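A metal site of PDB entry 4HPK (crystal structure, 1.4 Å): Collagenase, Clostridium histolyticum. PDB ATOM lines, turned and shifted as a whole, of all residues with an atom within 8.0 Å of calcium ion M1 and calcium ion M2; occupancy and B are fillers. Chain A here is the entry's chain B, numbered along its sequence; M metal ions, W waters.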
ATOM      1  N   GLU A   9       3.336 -14.198  -6.322  1.00  0.00           N
ATOM      2  CA  GLU A   9       3.957 -14.633  -7.570  1.00  0.00           C
ATOM      3  C   GLU A   9       5.369 -14.056  -7.682  1.00  0.00           C
ATOM      4  O   GLU A   9       5.691 -13.043  -7.056  1.00  0.00           O
ATOM      5  CB  GLU A   9       3.129 -14.155  -8.759  1.00  0.00           C
ATOM      6  CG  GLU A   9       2.972 -12.636  -8.827  1.00  0.00           C
ATOM      7  CD  GLU A   9       2.488 -12.124 -10.158  1.00  0.00           C
ATOM      8  OE1 GLU A   9       1.795 -11.074 -10.181  1.00  0.00           O
ATOM      9  OE2 GLU A   9       2.827 -12.733 -11.198  1.00  0.00           O
ATOM     10  N   LYS A  10       6.187 -14.696  -8.527  1.00  0.00           N
ATOM     11  CA  LYS A  10       7.560 -14.226  -8.777  1.00  0.00           C
ATOM     12  C   LYS A  10       7.801 -13.928 -10.269  1.00  0.00           C
ATOM     13  O   LYS A  10       8.050 -14.835 -11.053  1.00  0.00           O
ATOM     14  CB  LYS A  10       8.576 -15.263  -8.291  1.00  0.00           C
ATOM     15  CG  LYS A  10       8.451 -15.611  -6.815  1.00  0.00           C
ATOM     16  CD  LYS A  10       9.562 -16.533  -6.362  1.00  0.00           C
ATOM     17  CE  LYS A  10       9.502 -16.814  -4.872  1.00  0.00           C
ATOM     18  NZ  LYS A  10       8.374 -17.699  -4.518  1.00  0.00           N
ATOM     19  N   GLU A  11       7.710 -12.651 -10.643  1.00  0.00           N
ATOM     20  CA  GLU A  11       8.035 -12.235 -12.020  1.00  0.00           C
ATOM     21  C   GLU A  11       9.551 -12.316 -12.222  1.00  0.00           C
ATOM     22  O   GLU A  11      10.292 -12.171 -11.248  1.00  0.00           O
ATOM     23  CB  GLU A  11       7.597 -10.796 -12.270  1.00  0.00           C
ATOM     24  CG  GLU A  11       6.086 -10.584 -12.256  1.00  0.00           C
ATOM     25  CD  GLU A  11       5.366 -11.154 -13.476  1.00  0.00           C
ATOM     26  OE1 GLU A  11       6.018 -11.612 -14.456  1.00  0.00           O
ATOM     27  OE2 GLU A  11       4.113 -11.152 -13.431  1.00  0.00           O
ATOM     28  N   ASN A  12      10.034 -12.546 -13.450  1.00  0.00           N
ATOM     29  CA  ASN A  12       9.258 -12.802 -14.658  1.00  0.00           C
ATOM     30  C   ASN A  12       8.731 -14.237 -14.628  1.00  0.00           C
ATOM     31  O   ASN A  12       9.480 -15.170 -14.392  1.00  0.00           O
ATOM     32  CB  ASN A  12      10.178 -12.606 -15.885  1.00  0.00           C
ATOM     33  CG  ASN A  12       9.470 -12.768 -17.240  1.00  0.00           C
ATOM     34  OD1 ASN A  12       8.490 -13.477 -17.379  1.00  0.00           O
ATOM     35  ND2 ASN A  12      10.032 -12.119 -18.257  1.00  0.00           N
ATOM     36  N   ASN A  13       7.428 -14.403 -14.836  1.00  0.00           N
ATOM     37  CA  ASN A  13       6.818 -15.740 -14.908  1.00  0.00           C
ATOM     38  C   ASN A  13       5.970 -15.916 -16.168  1.00  0.00           C
ATOM     39  O   ASN A  13       4.975 -16.616 -16.152  1.00  0.00           O
ATOM     40  CB  ASN A  13       5.983 -16.010 -13.654  1.00  0.00           C
ATOM     41  CG  ASN A  13       4.923 -14.960 -13.435  1.00  0.00           C
ATOM     42  OD1 ASN A  13       4.596 -14.193 -14.345  1.00  0.00           O
ATOM     43  ND2 ASN A  13       4.396 -14.896 -12.215  1.00  0.00           N
ATOM     44  N   ASP A  14       6.378 -15.291 -17.276  1.00  0.00           N
ATOM     45  CA  ASP A  14       5.519 -15.231 -18.462  1.00  0.00           C
ATOM     46  C   ASP A  14       5.560 -16.482 -19.355  1.00  0.00           C
ATOM     47  O   ASP A  14       4.754 -16.602 -20.277  1.00  0.00           O
ATOM     48  CB  ASP A  14       5.843 -13.988 -19.293  1.00  0.00           C
ATOM     49  CG  ASP A  14       5.622 -12.691 -18.521  1.00  0.00           C
ATOM     50  OD1 ASP A  14       5.980 -11.625 -19.073  1.00  0.00           O
ATOM     51  OD2 ASP A  14       5.091 -12.705 -17.383  1.00  0.00           O
ATOM     52  N   SER A  15       6.480 -17.404 -19.079  1.00  0.00           N
ATOM     53  CA  SER A  15       6.563 -18.669 -19.834  1.00  0.00           C
ATOM     54  C   SER A  15       6.628 -19.856 -18.892  1.00  0.00           C
ATOM     55  O   SER A  15       6.888 -19.698 -17.698  1.00  0.00           O
ATOM     56  CB  SER A  15       7.804 -18.665 -20.720  1.00  0.00           C
ATOM     57  OG  SER A  15       8.982 -18.542 -19.941  1.00  0.00           O
ATOM     58  N   LYS A  18       9.612 -20.372 -16.695  1.00  0.00           N
ATOM     59  CA  LYS A  18       9.774 -19.386 -15.632  1.00  0.00           C
ATOM     60  C   LYS A  18       8.616 -19.412 -14.620  1.00  0.00           C
ATOM     61  O   LYS A  18       8.450 -18.491 -13.824  1.00  0.00           O
ATOM     62  CB  LYS A  18       9.883 -17.982 -16.242  1.00  0.00           C
ATOM     63  CG  LYS A  18      11.028 -17.801 -17.245  1.00  0.00           C
ATOM     64  CD  LYS A  18      10.951 -16.424 -17.905  1.00  0.00           C
ATOM     65  CE  LYS A  18      11.973 -16.273 -19.034  1.00  0.00           C
ATOM     66  NZ  LYS A  18      11.844 -14.947 -19.714  1.00  0.00           N
ATOM     67  N   THR A  20       6.052 -19.747 -11.562  1.00  0.00           N
ATOM     68  CA  THR A  20       6.148 -19.671 -10.106  1.00  0.00           C
ATOM     69  C   THR A  20       5.609 -20.956  -9.504  1.00  0.00           C
ATOM     70  O   THR A  20       4.489 -21.363  -9.790  1.00  0.00           O
ATOM     71  CB  THR A  20       5.347 -18.490  -9.545  1.00  0.00           C
ATOM     72  OG1 THR A  20       5.803 -17.270 -10.145  1.00  0.00           O
ATOM     73  CG2 THR A  20       5.465 -18.410  -8.021  1.00  0.00           C
ATOM     74  N   GLN A  30      -0.943 -14.928  -4.732  1.00  0.00           N
ATOM     75  CA  GLN A  30      -1.415 -13.577  -4.961  1.00  0.00           C
ATOM     76  C   GLN A  30      -0.690 -13.023  -6.156  1.00  0.00           C
ATOM     77  O   GLN A  30       0.532 -13.044  -6.205  1.00  0.00           O
ATOM     78  CB  GLN A  30      -1.153 -12.715  -3.736  1.00  0.00           C
ATOM     79  CG  GLN A  30      -1.911 -13.240  -2.526  1.00  0.00           C
ATOM     80  CD  GLN A  30      -1.597 -12.498  -1.243  1.00  0.00           C
ATOM     81  OE1 GLN A  30      -0.440 -12.262  -0.926  1.00  0.00           O
ATOM     82  NE2 GLN A  30      -2.642 -12.147  -0.508  1.00  0.00           N
ATOM     83  N   GLY A  31      -1.440 -12.554  -7.147  1.00  0.00           N
ATOM     84  CA  GLY A  31      -0.838 -12.042  -8.357  1.00  0.00           C
ATOM     85  C   GLY A  31      -1.569 -10.843  -8.925  1.00  0.00           C
ATOM     86  O   GLY A  31      -2.667 -10.476  -8.478  1.00  0.00           O
ATOM     87  N   SER A  32      -0.920 -10.226  -9.905  1.00  0.00           N
ATOM     88  CA  SER A  32      -1.511  -9.103 -10.610  1.00  0.00           C
ATOM     89  C   SER A  32      -1.171  -9.209 -12.070  1.00  0.00           C
ATOM     90  O   SER A  32      -0.101  -9.711 -12.453  1.00  0.00           O
ATOM     91  CB  SER A  32      -1.005  -7.758 -10.065  1.00  0.00           C
ATOM     92  OG  SER A  32       0.328  -7.510 -10.405  1.00  0.00           O
ATOM     93  N   LEU A  33      -2.097  -8.717 -12.903  1.00  0.00           N
ATOM     94  CA  LEU A  33      -1.916  -8.638 -14.341  1.00  0.00           C
ATOM     95  C   LEU A  33      -2.236  -7.209 -14.767  1.00  0.00           C
ATOM     96  O   LEU A  33      -3.286  -6.942 -15.339  1.00  0.00           O
ATOM     97  CB  LEU A  33      -2.835  -9.626 -15.046  1.00  0.00           C
ATOM     98  CG  LEU A  33      -2.441 -11.092 -14.815  1.00  0.00           C
ATOM     99  CD1 LEU A  33      -3.578 -11.978 -15.239  1.00  0.00           C
ATOM    100  CD2 LEU A  33      -1.162 -11.466 -15.559  1.00  0.00           C
ATOM    101  N   LEU A  34      -1.337  -6.282 -14.439  1.00  0.00           N
ATOM    102  CA  LEU A  34      -1.512  -4.861 -14.753  1.00  0.00           C
ATOM    103  C   LEU A  34      -0.793  -4.458 -16.032  1.00  0.00           C
ATOM    104  O   LEU A  34       0.357  -4.800 -16.237  1.00  0.00           O
ATOM    105  CB  LEU A  34      -0.964  -4.020 -13.590  1.00  0.00           C
ATOM    106  CG  LEU A  34      -1.480  -4.335 -12.200  1.00  0.00           C
ATOM    107  CD1 LEU A  34      -0.822  -3.385 -11.184  1.00  0.00           C
ATOM    108  CD2 LEU A  34      -2.993  -4.242 -12.090  1.00  0.00           C
ATOM    109  N   ASP A  36       0.884  -4.228 -19.429  1.00  0.00           N
ATOM    110  CA  ASP A  36       1.449  -5.209 -20.342  1.00  0.00           C
ATOM    111  C   ASP A  36       1.743  -6.570 -19.730  1.00  0.00           C
ATOM    112  O   ASP A  36       2.061  -7.500 -20.467  1.00  0.00           O
ATOM    113  CB  ASP A  36       2.707  -4.654 -21.019  1.00  0.00           C
ATOM    114  CG  ASP A  36       2.410  -3.502 -21.965  1.00  0.00           C
ATOM    115  OD1 ASP A  36       1.274  -3.389 -22.466  1.00  0.00           O
ATOM    116  OD2 ASP A  36       3.341  -2.715 -22.205  1.00  0.00           O
ATOM    117  N   ASP A  37       1.650  -6.708 -18.404  1.00  0.00           N
ATOM    118  CA  ASP A  37       1.773  -8.021 -17.781  1.00  0.00           C
ATOM    119  C   ASP A  37       0.447  -8.754 -17.946  1.00  0.00           C
ATOM    120  O   ASP A  37      -0.512  -8.462 -17.252  1.00  0.00           O
ATOM    121  CB  ASP A  37       2.144  -7.892 -16.295  1.00  0.00           C
ATOM    122  CG  ASP A  37       2.361  -9.244 -15.624  1.00  0.00           C
ATOM    123  OD1 ASP A  37       2.958 -10.151 -16.248  1.00  0.00           O
ATOM    124  OD2 ASP A  37       1.940  -9.395 -14.451  1.00  0.00           O
ATOM    125  N   SER A  38       0.403  -9.672 -18.904  1.00  0.00           N
ATOM    126  CA  SER A  38      -0.865 -10.324 -19.241  1.00  0.00           C
ATOM    127  C   SER A  38      -0.867 -11.830 -19.025  1.00  0.00           C
ATOM    128  O   SER A  38      -1.887 -12.466 -19.234  1.00  0.00           O
ATOM    129  CB  SER A  38      -1.254 -10.028 -20.681  1.00  0.00           C
ATOM    130  OG  SER A  38      -0.300 -10.599 -21.539  1.00  0.00           O
ATOM    131  N   ARG A  39       0.271 -12.375 -18.603  1.00  0.00           N
ATOM    132  CA  ARG A  39       0.390 -13.801 -18.334  1.00  0.00           C
ATOM    133  C   ARG A  39       1.228 -14.037 -17.090  1.00  0.00           C
ATOM    134  O   ARG A  39       2.324 -13.452 -16.950  1.00  0.00           O
ATOM    135  CB  ARG A  39       1.082 -14.516 -19.482  1.00  0.00           C
ATOM    136  CG  ARG A  39       0.444 -14.360 -20.851  1.00  0.00           C
ATOM    137  CD  ARG A  39       1.458 -14.597 -21.941  1.00  0.00           C
ATOM    138  NE  ARG A  39       2.152 -15.888 -21.822  1.00  0.00           N
ATOM    139  CZ  ARG A  39       1.777 -17.022 -22.427  1.00  0.00           C
ATOM    140  NH1 ARG A  39       0.694 -17.057 -23.189  1.00  0.00           N
ATOM    141  NH2 ARG A  39       2.505 -18.132 -22.261  1.00  0.00           N
ATOM    142  N   ASP A  40       0.725 -14.886 -16.204  1.00  0.00           N
ATOM    143  CA  ASP A  40       1.448 -15.361 -15.011  1.00  0.00           C
ATOM    144  C   ASP A  40       1.365 -16.879 -15.007  1.00  0.00           C
ATOM    145  O   ASP A  40       0.281 -17.453 -14.850  1.00  0.00           O
ATOM    146  CB  ASP A  40       0.793 -14.829 -13.720  1.00  0.00           C
ATOM    147  CG  ASP A  40       0.971 -13.317 -13.516  1.00  0.00           C
ATOM    148  OD1 ASP A  40       1.837 -12.697 -14.176  1.00  0.00           O
ATOM    149  OD2 ASP A  40       0.241 -12.748 -12.673  1.00  0.00           O
ATOM    150  N   TYR A  41       2.513 -17.529 -15.181  1.00  0.00           N
ATOM    151  CA  TYR A  41       2.589 -18.976 -15.236  1.00  0.00           C
ATOM    152  C   TYR A  41       2.935 -19.507 -13.833  1.00  0.00           C
ATOM    153  O   TYR A  41       3.804 -18.959 -13.147  1.00  0.00           O
ATOM    154  CB  TYR A  41       3.627 -19.453 -16.274  1.00  0.00           C
ATOM    155  CG  TYR A  41       3.099 -20.485 -17.258  1.00  0.00           C
ATOM    156  CD1 TYR A  41       3.246 -20.318 -18.630  1.00  0.00           C
ATOM    157  CD2 TYR A  41       2.408 -21.586 -16.800  1.00  0.00           C
ATOM    158  CE1 TYR A  41       2.750 -21.260 -19.522  1.00  0.00           C
ATOM    159  CE2 TYR A  41       1.894 -22.518 -17.683  1.00  0.00           C
ATOM    160  CZ  TYR A  41       2.071 -22.361 -19.043  1.00  0.00           C
ATOM    161  OH  TYR A  41       1.551 -23.305 -19.891  1.00  0.00           O
ATOM    162  N   TYR A  42       2.214 -20.555 -13.436  1.00  0.00           N
ATOM    163  CA  TYR A  42       2.458 -21.287 -12.206  1.00  0.00           C
ATOM    164  C   TYR A  42       2.703 -22.768 -12.529  1.00  0.00           C
ATOM    165  O   TYR A  42       2.344 -23.254 -13.590  1.00  0.00           O
ATOM    166  CB  TYR A  42       1.255 -21.168 -11.268  1.00  0.00           C
ATOM    167  CG  TYR A  42       0.989 -19.762 -10.826  1.00  0.00           C
ATOM    168  CD1 TYR A  42       0.149 -18.926 -11.554  1.00  0.00           C
ATOM    169  CD2 TYR A  42       1.579 -19.252  -9.668  1.00  0.00           C
ATOM    170  CE1 TYR A  42      -0.090 -17.629 -11.137  1.00  0.00           C
ATOM    171  CE2 TYR A  42       1.339 -17.963  -9.245  1.00  0.00           C
ATOM    172  CZ  TYR A  42       0.514 -17.146  -9.978  1.00  0.00           C
ATOM    173  OH  TYR A  42       0.275 -15.857  -9.538  1.00  0.00           O
ATOM    174  N   LEU A 102      -1.406 -21.680 -16.448  1.00  0.00           N
ATOM    175  CA  LEU A 102      -1.211 -20.360 -17.007  1.00  0.00           C
ATOM    176  C   LEU A 102      -2.430 -19.517 -16.677  1.00  0.00           C
ATOM    177  O   LEU A 102      -3.542 -19.849 -17.103  1.00  0.00           O
ATOM    178  CB  LEU A 102      -1.052 -20.448 -18.537  1.00  0.00           C
ATOM    179  CG  LEU A 102      -1.020 -19.107 -19.287  1.00  0.00           C
ATOM    180  CD1 LEU A 102       0.164 -18.252 -18.838  1.00  0.00           C
ATOM    181  CD2 LEU A 102      -1.007 -19.359 -20.805  1.00  0.00           C
ATOM    182  N   VAL A 103      -2.219 -18.452 -15.919  1.00  0.00           N
ATOM    183  CA  VAL A 103      -3.241 -17.424 -15.702  1.00  0.00           C
ATOM    184  C   VAL A 103      -2.978 -16.308 -16.711  1.00  0.00           C
ATOM    185  O   VAL A 103      -1.874 -15.784 -16.788  1.00  0.00           O
ATOM    186  CB  VAL A 103      -3.186 -16.877 -14.251  1.00  0.00           C
ATOM    187  CG1 VAL A 103      -4.234 -15.787 -14.042  1.00  0.00           C
ATOM    188  CG2 VAL A 103      -3.407 -18.008 -13.232  1.00  0.00           C
ATOM    189  N   GLY A 110      -6.005  -6.144 -13.537  1.00  0.00           N
ATOM    190  CA  GLY A 110      -6.399  -6.340 -12.166  1.00  0.00           C
ATOM    191  C   GLY A 110      -5.571  -7.366 -11.434  1.00  0.00           C
ATOM    192  O   GLY A 110      -4.635  -7.954 -11.975  1.00  0.00           O
ATOM    193  N   ASN A 111      -5.971  -7.565 -10.179  1.00  0.00           N
ATOM    194  CA  ASN A 111      -5.335  -8.495  -9.259  1.00  0.00           C
ATOM    195  C   ASN A 111      -6.226  -9.698  -9.044  1.00  0.00           C
ATOM    196  O   ASN A 111      -7.438  -9.670  -9.295  1.00  0.00           O
ATOM    197  CB  ASN A 111      -5.092  -7.816  -7.912  1.00  0.00           C
ATOM    198  CG  ASN A 111      -4.168  -6.620  -8.016  1.00  0.00           C
ATOM    199  OD1 ASN A 111      -3.364  -6.524  -8.935  1.00  0.00           O
ATOM    200  ND2 ASN A 111      -4.292  -5.702  -7.063  1.00  0.00           N
ATOM    201  N   TYR A 112      -5.622 -10.792  -8.583  1.00  0.00           N
ATOM    202  CA  TYR A 112      -6.332 -12.033  -8.381  1.00  0.00           C
ATOM    203  C   TYR A 112      -5.627 -12.854  -7.291  1.00  0.00           C
ATOM    204  O   TYR A 112      -4.485 -12.574  -6.932  1.00  0.00           O
ATOM    205  CB  TYR A 112      -6.402 -12.843  -9.700  1.00  0.00           C
ATOM    206  CG  TYR A 112      -5.043 -13.276 -10.173  1.00  0.00           C
ATOM    207  CD1 TYR A 112      -4.476 -14.468  -9.727  1.00  0.00           C
ATOM    208  CD2 TYR A 112      -4.284 -12.457 -10.976  1.00  0.00           C
ATOM    209  CE1 TYR A 112      -3.202 -14.839 -10.118  1.00  0.00           C
ATOM    210  CE2 TYR A 112      -3.004 -12.813 -11.360  1.00  0.00           C
ATOM    211  CZ  TYR A 112      -2.463 -14.008 -10.929  1.00  0.00           C
ATOM    212  OH  TYR A 112      -1.186 -14.380 -11.303  1.00  0.00           O
HETATM  213 CA    CA M   1       3.765 -12.332 -15.496  1.00  0.00          CA
HETATM  214 CA    CA M   2       1.959 -10.808 -12.596  1.00  0.00          CA
HETATM  215  O   HOH W   1       3.026  -8.807 -11.731  1.00  0.00           O
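The backbone NH (N) of Asp 14 sits at hydrogen-bond distance from the side-chain amide oxygen (OD1) of Asn 12 (2.8 Å). The side-chain carboxylate (OE2) of Glu 9 lies close to the side-chain amide nitrogen (ND2) of Asn 13, at 2.9 Å. N of Tyr 41 sits at hydrogen-bond distance from O of Asn 13 (2.8 Å). The backbone NH (N) of Glu 9 lies within hydrogen-bond range of the backbone carbonyl oxygen (O) of Gln 30, 3.0 Å away. The backbone NH (N) of Asp 40 is in hydrogen-bond range of the backbone carbonyl oxygen (O) of Val 103 (2.8 Å). OH of Tyr 112 lies close to OD2 of Asp 40 (2.6 Å). The side-chain amide nitrogen of Asn 13 is in hydrogen-bond range of the side-chain hydroxyl of Thr 20 (3.4 Å).
Within 4 Å of calcium ion M1: Glu 11, Asn 13, Asp 14, Asp 37, Arg 39 and Asp 40. The nearest printed residue that does not touch calcium ion M1 is Glu 9 (4.4 Å).
Within 4 Å of calcium ion M2: Glu 9, Glu 11, Ser 32, Asp 37 and Asp 40.
O of Arg 39 binds calcium ion M1 (2.3 Å). OD2 of Asp 14 binds calcium ion M1 (2.3 Å). OD1 of Asn 13 is bound to calcium ion M1, at 2.3 Å. Calcium ion M1 is bound by OD1 of Asp 40, at 2.4 Å. OE2 of Glu 11 is bound to calcium ion M1, at 2.4 Å. Calcium ion M1 is bound by the side-chain carboxylate (OD1) of Asp 37, at 2.4 Å. The side-chain carboxylate (OE1) of Glu 11 binds calcium ion M1 (2.6 Å). Calcium ion M1 has seven donor atoms within binding distance.
Calcium ion M2 is bound by OD2 of Asp 37 (2.3 Å), OE2 of Glu 11 (2.3 Å), O of Ser 32 (2.3 Å), water W1 (2.4 Å), OE1 of Glu 9 (2.4 Å), OD1 of Asp 40 (2.5 Å), OE2 of Glu 9 (2.5 Å) and OD2 of Asp 40 (2.6 Å).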
